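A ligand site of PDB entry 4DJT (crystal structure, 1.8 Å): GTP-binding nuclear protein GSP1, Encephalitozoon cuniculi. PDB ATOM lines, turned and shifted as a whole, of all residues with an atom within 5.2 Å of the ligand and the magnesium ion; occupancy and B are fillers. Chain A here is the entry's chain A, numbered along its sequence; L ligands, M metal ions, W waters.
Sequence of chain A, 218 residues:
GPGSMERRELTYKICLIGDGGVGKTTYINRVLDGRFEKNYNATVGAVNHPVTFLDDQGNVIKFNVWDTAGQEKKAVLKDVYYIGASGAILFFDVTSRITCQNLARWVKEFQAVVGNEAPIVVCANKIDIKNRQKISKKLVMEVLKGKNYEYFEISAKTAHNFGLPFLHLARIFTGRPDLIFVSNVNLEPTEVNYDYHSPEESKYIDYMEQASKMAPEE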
ATOM      1  N   ASP A  19      20.533  -0.711  14.960  1.00  0.00           N
ATOM      2  CA  ASP A  19      20.327  -0.040  16.239  1.00  0.00           C
ATOM      3  C   ASP A  19      19.115   0.890  16.228  1.00  0.00           C
ATOM      4  O   ASP A  19      18.715   1.399  15.188  1.00  0.00           O
ATOM      5  CB  ASP A  19      21.542   0.768  16.638  1.00  0.00           C
ATOM      6  CG  ASP A  19      22.669  -0.093  17.210  1.00  0.00           C
ATOM      7  OD1 ASP A  19      22.560  -1.359  17.284  1.00  0.00           O
ATOM      8  OD2 ASP A  19      23.651   0.535  17.600  1.00  0.00           O
ATOM      9  N   GLY A  20      18.584   1.140  17.410  1.00  0.00           N
ATOM     10  CA  GLY A  20      17.605   2.181  17.575  1.00  0.00           C
ATOM     11  C   GLY A  20      18.140   3.494  17.030  1.00  0.00           C
ATOM     12  O   GLY A  20      19.337   3.858  17.231  1.00  0.00           O
ATOM     13  N   GLY A  21      17.299   4.198  16.293  1.00  0.00           N
ATOM     14  CA  GLY A  21      17.619   5.535  15.850  1.00  0.00           C
ATOM     15  C   GLY A  21      18.236   5.621  14.468  1.00  0.00           C
ATOM     16  O   GLY A  21      18.443   6.738  13.971  1.00  0.00           O
ATOM     17  N   VAL A  22      18.495   4.468  13.817  1.00  0.00           N
ATOM     18  CA  VAL A  22      19.253   4.464  12.555  1.00  0.00           C
ATOM     19  C   VAL A  22      18.390   4.755  11.343  1.00  0.00           C
ATOM     20  O   VAL A  22      18.926   5.076  10.290  1.00  0.00           O
ATOM     21  CB  VAL A  22      20.046   3.168  12.304  1.00  0.00           C
ATOM     22  CG1 VAL A  22      21.025   2.900  13.459  1.00  0.00           C
ATOM     23  CG2 VAL A  22      19.111   1.977  12.121  1.00  0.00           C
ATOM     24  N   GLY A  23      17.054   4.631  11.490  1.00  0.00           N
ATOM     25  CA  GLY A  23      16.097   4.992  10.437  1.00  0.00           C
ATOM     26  C   GLY A  23      15.268   3.819   9.858  1.00  0.00           C
ATOM     27  O   GLY A  23      14.709   3.965   8.800  1.00  0.00           O
ATOM     28  N   LYS A  24      15.232   2.668  10.533  1.00  0.00           N
ATOM     29  CA  LYS A  24      14.454   1.517  10.049  1.00  0.00           C
ATOM     30  C   LYS A  24      12.991   1.881   9.781  1.00  0.00           C
ATOM     31  O   LYS A  24      12.447   1.595   8.696  1.00  0.00           O
ATOM     32  CB  LYS A  24      14.530   0.375  11.054  1.00  0.00           C
ATOM     33  CG  LYS A  24      15.953  -0.110  11.311  1.00  0.00           C
ATOM     34  CD  LYS A  24      15.991  -1.264  12.290  1.00  0.00           C
ATOM     35  CE  LYS A  24      15.369  -0.943  13.652  1.00  0.00           C
ATOM     36  NZ  LYS A  24      16.166   0.054  14.426  1.00  0.00           N
ATOM     37  N   THR A  25      12.346   2.495  10.776  1.00  0.00           N
ATOM     38  CA  THR A  25      10.937   2.832  10.657  1.00  0.00           C
ATOM     39  C   THR A  25      10.692   3.915   9.619  1.00  0.00           C
ATOM     40  O   THR A  25       9.760   3.808   8.799  1.00  0.00           O
ATOM     41  CB  THR A  25      10.382   3.221  12.057  1.00  0.00           C
ATOM     42  OG1 THR A  25      10.563   2.103  12.938  1.00  0.00           O
ATOM     43  CG2 THR A  25       8.919   3.566  11.970  1.00  0.00           C
ATOM     44  N   THR A  26      11.578   4.909   9.573  1.00  0.00           N
ATOM     45  CA  THR A  26      11.476   5.963   8.550  1.00  0.00           C
ATOM     46  C   THR A  26      11.515   5.376   7.128  1.00  0.00           C
ATOM     47  O   THR A  26      10.759   5.811   6.225  1.00  0.00           O
ATOM     48  CB  THR A  26      12.534   7.078   8.738  1.00  0.00           C
ATOM     49  OG1 THR A  26      12.411   7.607  10.084  1.00  0.00           O
ATOM     50  CG2 THR A  26      12.323   8.220   7.726  1.00  0.00           C
ATOM     51  N   TYR A  27      12.363   4.371   6.950  1.00  0.00           N
ATOM     52  CA  TYR A  27      12.509   3.681   5.690  1.00  0.00           C
ATOM     53  C   TYR A  27      11.225   3.005   5.263  1.00  0.00           C
ATOM     54  O   TYR A  27      10.712   3.275   4.184  1.00  0.00           O
ATOM     55  CB  TYR A  27      13.606   2.651   5.776  1.00  0.00           C
ATOM     56  CG  TYR A  27      13.855   1.861   4.488  1.00  0.00           C
ATOM     57  CD1 TYR A  27      14.463   2.460   3.387  1.00  0.00           C
ATOM     58  CD2 TYR A  27      13.566   0.522   4.421  1.00  0.00           C
ATOM     59  CE1 TYR A  27      14.727   1.734   2.242  1.00  0.00           C
ATOM     60  CE2 TYR A  27      13.838  -0.218   3.279  1.00  0.00           C
ATOM     61  CZ  TYR A  27      14.411   0.409   2.184  1.00  0.00           C
ATOM     62  OH  TYR A  27      14.680  -0.354   1.043  1.00  0.00           O
ATOM     63  N   ASP A  67       9.199  -4.767  10.966  1.00  0.00           N
ATOM     64  CA  ASP A  67       9.886  -3.648  11.656  1.00  0.00           C
ATOM     65  C   ASP A  67       9.571  -3.793  13.111  1.00  0.00           C
ATOM     66  O   ASP A  67       8.469  -4.244  13.452  1.00  0.00           O
ATOM     67  CB  ASP A  67       9.334  -2.311  11.160  1.00  0.00           C
ATOM     68  CG  ASP A  67      10.056  -1.104  11.744  1.00  0.00           C
ATOM     69  OD1 ASP A  67      11.251  -1.244  12.052  1.00  0.00           O
ATOM     70  OD2 ASP A  67       9.442   0.024  11.813  1.00  0.00           O
ATOM     71  N   THR A  68      10.469  -3.350  13.979  1.00  0.00           N
ATOM     72  CA  THR A  68      10.225  -3.394  15.399  1.00  0.00           C
ATOM     73  C   THR A  68       9.346  -2.207  15.829  1.00  0.00           C
ATOM     74  O   THR A  68       9.085  -1.297  15.066  1.00  0.00           O
ATOM     75  CB  THR A  68      11.509  -3.282  16.228  1.00  0.00           C
ATOM     76  OG1 THR A  68      11.970  -1.920  16.210  1.00  0.00           O
ATOM     77  CG2 THR A  68      12.564  -4.242  15.736  1.00  0.00           C
ATOM     78  N   GLY A  70      10.430  -0.496  18.481  1.00  0.00           N
ATOM     79  CA  GLY A  70      11.401   0.285  19.196  1.00  0.00           C
ATOM     80  C   GLY A  70      12.101  -0.463  20.331  1.00  0.00           C
ATOM     81  O   GLY A  70      13.021   0.080  20.954  1.00  0.00           O
ATOM     82  N   GLU A  72      14.348  -2.661  20.507  1.00  0.00           N
ATOM     83  CA  GLU A  72      15.800  -2.835  20.332  1.00  0.00           C
ATOM     84  C   GLU A  72      16.630  -1.766  21.060  1.00  0.00           C
ATOM     85  O   GLU A  72      17.811  -1.960  21.275  1.00  0.00           O
ATOM     86  CB  GLU A  72      16.234  -2.878  18.837  1.00  0.00           C
ATOM     87  CG  GLU A  72      16.227  -1.548  18.067  1.00  0.00           C
ATOM     88  CD  GLU A  72      14.839  -1.126  17.594  1.00  0.00           C
ATOM     89  OE1 GLU A  72      13.831  -1.747  18.031  1.00  0.00           O
ATOM     90  OE2 GLU A  72      14.774  -0.185  16.814  1.00  0.00           O
ATOM     91  N   LYS A  73      15.995  -0.665  21.432  1.00  0.00           N
ATOM     92  CA  LYS A  73      16.676   0.427  22.110  1.00  0.00           C
ATOM     93  C   LYS A  73      17.139   0.003  23.488  1.00  0.00           C
ATOM     94  O   LYS A  73      18.202   0.418  23.931  1.00  0.00           O
ATOM     95  CB  LYS A  73      15.768   1.652  22.236  1.00  0.00           C
ATOM     96  CG  LYS A  73      15.429   2.295  20.909  1.00  0.00           C
ATOM     97  CD  LYS A  73      14.523   3.493  21.066  1.00  0.00           C
ATOM     98  CE  LYS A  73      14.092   4.031  19.719  1.00  0.00           C
ATOM     99  NZ  LYS A  73      13.100   5.124  19.878  1.00  0.00           N
ATOM    100  N   ASN A 125      22.459   4.648   6.080  1.00  0.00           N
ATOM    101  CA  ASN A 125      21.352   5.590   6.064  1.00  0.00           C
ATOM    102  C   ASN A 125      21.739   6.992   6.568  1.00  0.00           C
ATOM    103  O   ASN A 125      22.733   7.156   7.286  1.00  0.00           O
ATOM    104  CB  ASN A 125      20.173   5.025   6.872  1.00  0.00           C
ATOM    105  CG  ASN A 125      18.914   5.860   6.728  1.00  0.00           C
ATOM    106  OD1 ASN A 125      18.583   6.294   5.621  1.00  0.00           O
ATOM    107  ND2 ASN A 125      18.144   6.020   7.857  1.00  0.00           N
ATOM    108  N   LYS A 126      20.928   7.979   6.171  1.00  0.00           N
ATOM    109  CA  LYS A 126      21.076   9.382   6.600  1.00  0.00           C
ATOM    110  C   LYS A 126      22.230  10.029   5.869  1.00  0.00           C
ATOM    111  O   LYS A 126      22.841  10.993   6.377  1.00  0.00           O
ATOM    112  CB  LYS A 126      21.279   9.489   8.104  1.00  0.00           C
ATOM    113  CG  LYS A 126      20.203   8.837   8.926  1.00  0.00           C
ATOM    114  CD  LYS A 126      20.182   9.345  10.340  1.00  0.00           C
ATOM    115  CE  LYS A 126      19.263   8.550  11.242  1.00  0.00           C
ATOM    116  NZ  LYS A 126      19.402   8.914  12.690  1.00  0.00           N
ATOM    117  N   ASP A 128      22.027  12.033   3.805  1.00  0.00           N
ATOM    118  CA  ASP A 128      21.639  13.444   3.643  1.00  0.00           C
ATOM    119  C   ASP A 128      22.242  14.407   4.679  1.00  0.00           C
ATOM    120  O   ASP A 128      22.261  15.601   4.444  1.00  0.00           O
ATOM    121  CB  ASP A 128      20.141  13.589   3.639  1.00  0.00           C
ATOM    122  CG  ASP A 128      19.483  13.063   4.918  1.00  0.00           C
ATOM    123  OD1 ASP A 128      19.258  11.828   5.008  1.00  0.00           O
ATOM    124  OD2 ASP A 128      19.159  13.901   5.811  1.00  0.00           O
ATOM    125  N   ILE A 129      22.752  13.912   5.804  1.00  0.00           N
ATOM    126  CA  ILE A 129      23.216  14.786   6.878  1.00  0.00           C
ATOM    127  C   ILE A 129      24.627  15.303   6.605  1.00  0.00           C
ATOM    128  O   ILE A 129      25.341  14.741   5.775  1.00  0.00           O
ATOM    129  CB  ILE A 129      23.199  14.100   8.255  1.00  0.00           C
ATOM    130  CG1 ILE A 129      21.788  13.639   8.601  1.00  0.00           C
ATOM    131  CG2 ILE A 129      23.687  15.053   9.344  1.00  0.00           C
ATOM    132  CD1 ILE A 129      21.638  13.075   9.998  1.00  0.00           C
ATOM    133  N   ILE A 154      21.680   5.197   1.292  1.00  0.00           N
ATOM    134  CA  ILE A 154      20.268   5.633   1.133  1.00  0.00           C
ATOM    135  C   ILE A 154      19.950   6.832   2.049  1.00  0.00           C
ATOM    136  O   ILE A 154      20.647   7.098   3.029  1.00  0.00           O
ATOM    137  CB  ILE A 154      19.234   4.517   1.482  1.00  0.00           C
ATOM    138  CG1 ILE A 154      19.273   4.169   2.955  1.00  0.00           C
ATOM    139  CG2 ILE A 154      19.507   3.197   0.701  1.00  0.00           C
ATOM    140  CD1 ILE A 154      18.147   3.204   3.412  1.00  0.00           C
ATOM    141  N   SER A 155      18.833   7.472   1.769  1.00  0.00           N
ATOM    142  CA  SER A 155      18.169   8.355   2.732  1.00  0.00           C
ATOM    143  C   SER A 155      16.734   7.881   2.951  1.00  0.00           C
ATOM    144  O   SER A 155      15.895   7.976   2.088  1.00  0.00           O
ATOM    145  CB  SER A 155      18.191   9.828   2.288  1.00  0.00           C
ATOM    146  OG  SER A 155      17.339  10.600   3.148  1.00  0.00           O
ATOM    147  N   ALA A 156      16.479   7.305   4.116  1.00  0.00           N
ATOM    148  CA  ALA A 156      15.127   6.870   4.425  1.00  0.00           C
ATOM    149  C   ALA A 156      14.172   8.045   4.441  1.00  0.00           C
ATOM    150  O   ALA A 156      13.004   7.884   4.182  1.00  0.00           O
ATOM    151  CB  ALA A 156      15.119   6.155   5.764  1.00  0.00           C
ATOM    152  N   LYS A 157      14.665   9.234   4.794  1.00  0.00           N
ATOM    153  CA  LYS A 157      13.808  10.454   4.811  1.00  0.00           C
ATOM    154  C   LYS A 157      13.191  10.733   3.432  1.00  0.00           C
ATOM    155  O   LYS A 157      11.955  10.851   3.308  1.00  0.00           O
ATOM    156  CB  LYS A 157      14.593  11.668   5.279  1.00  0.00           C
ATOM    157  CG  LYS A 157      13.827  12.997   5.139  1.00  0.00           C
ATOM    158  CD  LYS A 157      14.612  14.181   5.694  1.00  0.00           C
ATOM    159  CE  LYS A 157      15.744  14.629   4.775  1.00  0.00           C
ATOM    160  NZ  LYS A 157      15.366  15.789   3.902  1.00  0.00           N
ATOM    161  N   ASP A 195       5.329   3.030  17.567  1.00  0.00           N
ATOM    162  CA  ASP A 195       6.466   2.797  18.430  1.00  0.00           C
ATOM    163  C   ASP A 195       6.004   2.831  19.890  1.00  0.00           C
ATOM    164  O   ASP A 195       5.224   3.682  20.287  1.00  0.00           O
ATOM    165  CB  ASP A 195       7.531   3.894  18.271  1.00  0.00           C
ATOM    166  CG  ASP A 195       8.256   3.849  16.969  1.00  0.00           C
ATOM    167  OD1 ASP A 195       7.977   2.985  16.116  1.00  0.00           O
ATOM    168  OD2 ASP A 195       9.159   4.676  16.815  1.00  0.00           O
HETATM  169  P1  LIG L   1      14.638   3.401  14.008  1.00  0.00           P
HETATM  170  O1  LIG L   1      13.286   2.842  13.557  1.00  0.00           O
HETATM  171  O2  LIG L   1      15.844   2.715  13.390  1.00  0.00           O
HETATM  172  O3  LIG L   1      14.703   3.605  15.519  1.00  0.00           O
HETATM  173  O4  LIG L   1      14.748   4.933  13.494  1.00  0.00           O
HETATM  174  P2  LIG L   1      13.598   5.955  13.118  1.00  0.00           P
HETATM  175  O5  LIG L   1      13.014   5.683  11.740  1.00  0.00           O
HETATM  176  O6  LIG L   1      12.673   6.053  14.288  1.00  0.00           O
HETATM  177  O7  LIG L   1      14.343   7.337  12.945  1.00  0.00           O
HETATM  178  C1  LIG L   1      15.170   7.808  14.025  1.00  0.00           C
HETATM  179  C2  LIG L   1      15.399   9.293  13.812  1.00  0.00           C
HETATM  180  O8  LIG L   1      16.228   9.468  12.688  1.00  0.00           O
HETATM  181  C3  LIG L   1      14.141  10.043  13.513  1.00  0.00           C
HETATM  182  O9  LIG L   1      14.245  11.337  14.072  1.00  0.00           O
HETATM  183  C4  LIG L   1      14.099  10.189  12.018  1.00  0.00           C
HETATM  184  O10 LIG L   1      13.427  11.371  11.547  1.00  0.00           O
HETATM  185  C5  LIG L   1      15.579  10.230  11.712  1.00  0.00           C
HETATM  186  N1  LIG L   1      15.856   9.661  10.397  1.00  0.00           N
HETATM  187  C6  LIG L   1      15.550   8.429   9.925  1.00  0.00           C
HETATM  188  N2  LIG L   1      15.982   8.318   8.643  1.00  0.00           N
HETATM  189  C7  LIG L   1      16.611   9.446   8.321  1.00  0.00           C
HETATM  190  C8  LIG L   1      17.319   9.980   7.143  1.00  0.00           C
HETATM  191  O11 LIG L   1      17.451   9.301   6.081  1.00  0.00           O
HETATM  192  N3  LIG L   1      17.825  11.220   7.239  1.00  0.00           N
HETATM  193  C9  LIG L   1      17.696  11.981   8.364  1.00  0.00           C
HETATM  194  N4  LIG L   1      18.211  13.210   8.408  1.00  0.00           N
HETATM  195  N5  LIG L   1      17.064  11.553   9.475  1.00  0.00           N
HETATM  196  C10 LIG L   1      16.516  10.316   9.487  1.00  0.00           C
HETATM  197 MG    MG M   1      11.697   1.975  14.674  1.00  0.00          MG
HETATM  198  O   HOH W   1      13.907   5.552  16.996  1.00  0.00           O
HETATM  199  O   HOH W   2      11.252   3.957  15.220  1.00  0.00           O
HETATM  200  O   HOH W   3      12.946   1.655  16.403  1.00  0.00           O
HETATM  201  O   HOH W   4      12.149   0.006  14.100  1.00  0.00           O
HETATM  202  O   HOH W   5      14.212  13.888  12.107  1.00  0.00           O
HETATM  203  O   HOH W   6      10.041   1.272  15.622  1.00  0.00           O
HETATM  204  O   HOH W   7      10.553   7.694  13.842  1.00  0.00           O
HETATM  205  O   HOH W   8      18.876  11.609  12.895  1.00  0.00           O
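Water W4 lies within hydrogen-bond range of the side-chain carboxylate of Asp 67 and the side-chain hydroxyl of Thr 68. Water W6 lies within hydrogen-bond range of the side-chain carboxylate of Asp 195 (2.7 Å), the backbone carbonyl oxygen of Thr 68 (2.8 Å) and the backbone NH of Gly 70 (3.4 Å). Water W2 lies within hydrogen-bond range of an oxygen (O6) of the ligand (2.7 Å) and the side-chain carboxylate of Asp 195 (2.7 Å). Water W3 bridges OE2 of Glu 72 and O3 of the ligand. Water W1 bridges O3 of the ligand and NZ of Lys 73. Water W8 lies within hydrogen-bond range of the side-chain amino group (NZ) of Lys 126 (2.8 Å) and an oxygen (O8) of the ligand (3.4 Å).
N of Thr 25 sits at hydrogen-bond distance from O5 of the ligand, 3.4 Å away. N of Thr 26 is in hydrogen-bond range of O5 of the ligand, 2.7 Å away. OG1 of Thr 26 is in hydrogen-bond range of O5 of the ligand, 2.6 Å away. N3 of the ligand lies within hydrogen-bond range of OD1 of Asp 128 (2.7 Å). The backbone NH of Gly 21 sits at hydrogen-bond distance from an oxygen (O3) of the ligand, 2.8 Å away. O2 of the ligand sits at hydrogen-bond distance from N of Lys 24, 2.9 Å away. NZ of Lys 24 lies within salt-bridge range of O2 of the ligand, at 2.9 Å. N of Gly 23 sits at hydrogen-bond distance from O2 of the ligand (3.0 Å). The backbone NH (N) of Ala 156 sits at hydrogen-bond distance from an oxygen (O11) of the ligand, at 3.0 Å. N of Lys 157 is in hydrogen-bond range of O11 of the ligand, at 3.1 Å. N of Val 22 is in hydrogen-bond range of O2 of the ligand (3.2 Å). The side-chain hydroxyl (OG) of Ser 155 sits at hydrogen-bond distance from an oxygen (O11) of the ligand. An oxygen (O8) of the ligand is in hydrogen-bond range of the side-chain amino group (NZ) of Lys 126 (3.2 Å). OD1 of Asn 125 sits close to O11 of the ligand.
Of the 23 residues printed, 1 comes within 4 Å of the magnesium ion. The nearest printed residue that does not touch the magnesium ion is Asp 195 (4.1 Å).
Residues that only touch the ligand: Ile 129 (3.6 Å), Asp 19 (3.6 Å) and Gly 20 (3.8 Å). Hydrophobic or aromatic side chains that line the ligand: Val 22, Ile 129 and Ala 156. Within 4 Å of the ligand: Asp 19, Gly 20, Gly 21, Val 22, Gly 23, Lys 24, Thr 25, Thr 26, Asn 125, Lys 126, Asp 128, Ile 129, Ser 155, Ala 156 and Lys 157. The nearest printed residue that does not touch the ligand is Glu 72 (4.01 Å).
The side-chain hydroxyl (OG1) of Thr 25 sits close to the side-chain carboxylate (OD2) of Asp 67, at 2.6 Å. The side-chain carboxylate (OD1) of Asp 128 is in hydrogen-bond range of the side-chain hydroxyl (OG) of Ser 155 (2.9 Å). The side-chain amino group of Lys 126 sits at hydrogen-bond distance from the backbone carbonyl oxygen of Gly 21. O of Asp 19 lies within hydrogen-bond range of NZ of Lys 24, at 3.0 Å. The side-chain carboxylate (OE2) of Glu 72 lies within salt-bridge range of the side-chain amino group (NZ) of Lys 24, 2.8 Å away. The side-chain hydroxyl (OG) of Ser 155 sits close to the backbone NH (N) of Lys 157, at 3.4 Å. The backbone NH (N) of Lys 126 lies within hydrogen-bond range of the backbone carbonyl oxygen (O) of Ile 154 (3.3 Å). The side-chain amide oxygen of Asn 125 sits close to the backbone carbonyl oxygen of Ile 154 (3.4 Å).
The magnesium ion is bound by water W6 (2.0 Å), OG1 of Thr 25 (2.1 Å), water W4 (2.1 Å), water W2 (2.1 Å), O1 of the ligand (2.1 Å) and water W3 (2.2 Å). The magnesium ion has six donor atoms within binding distance.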
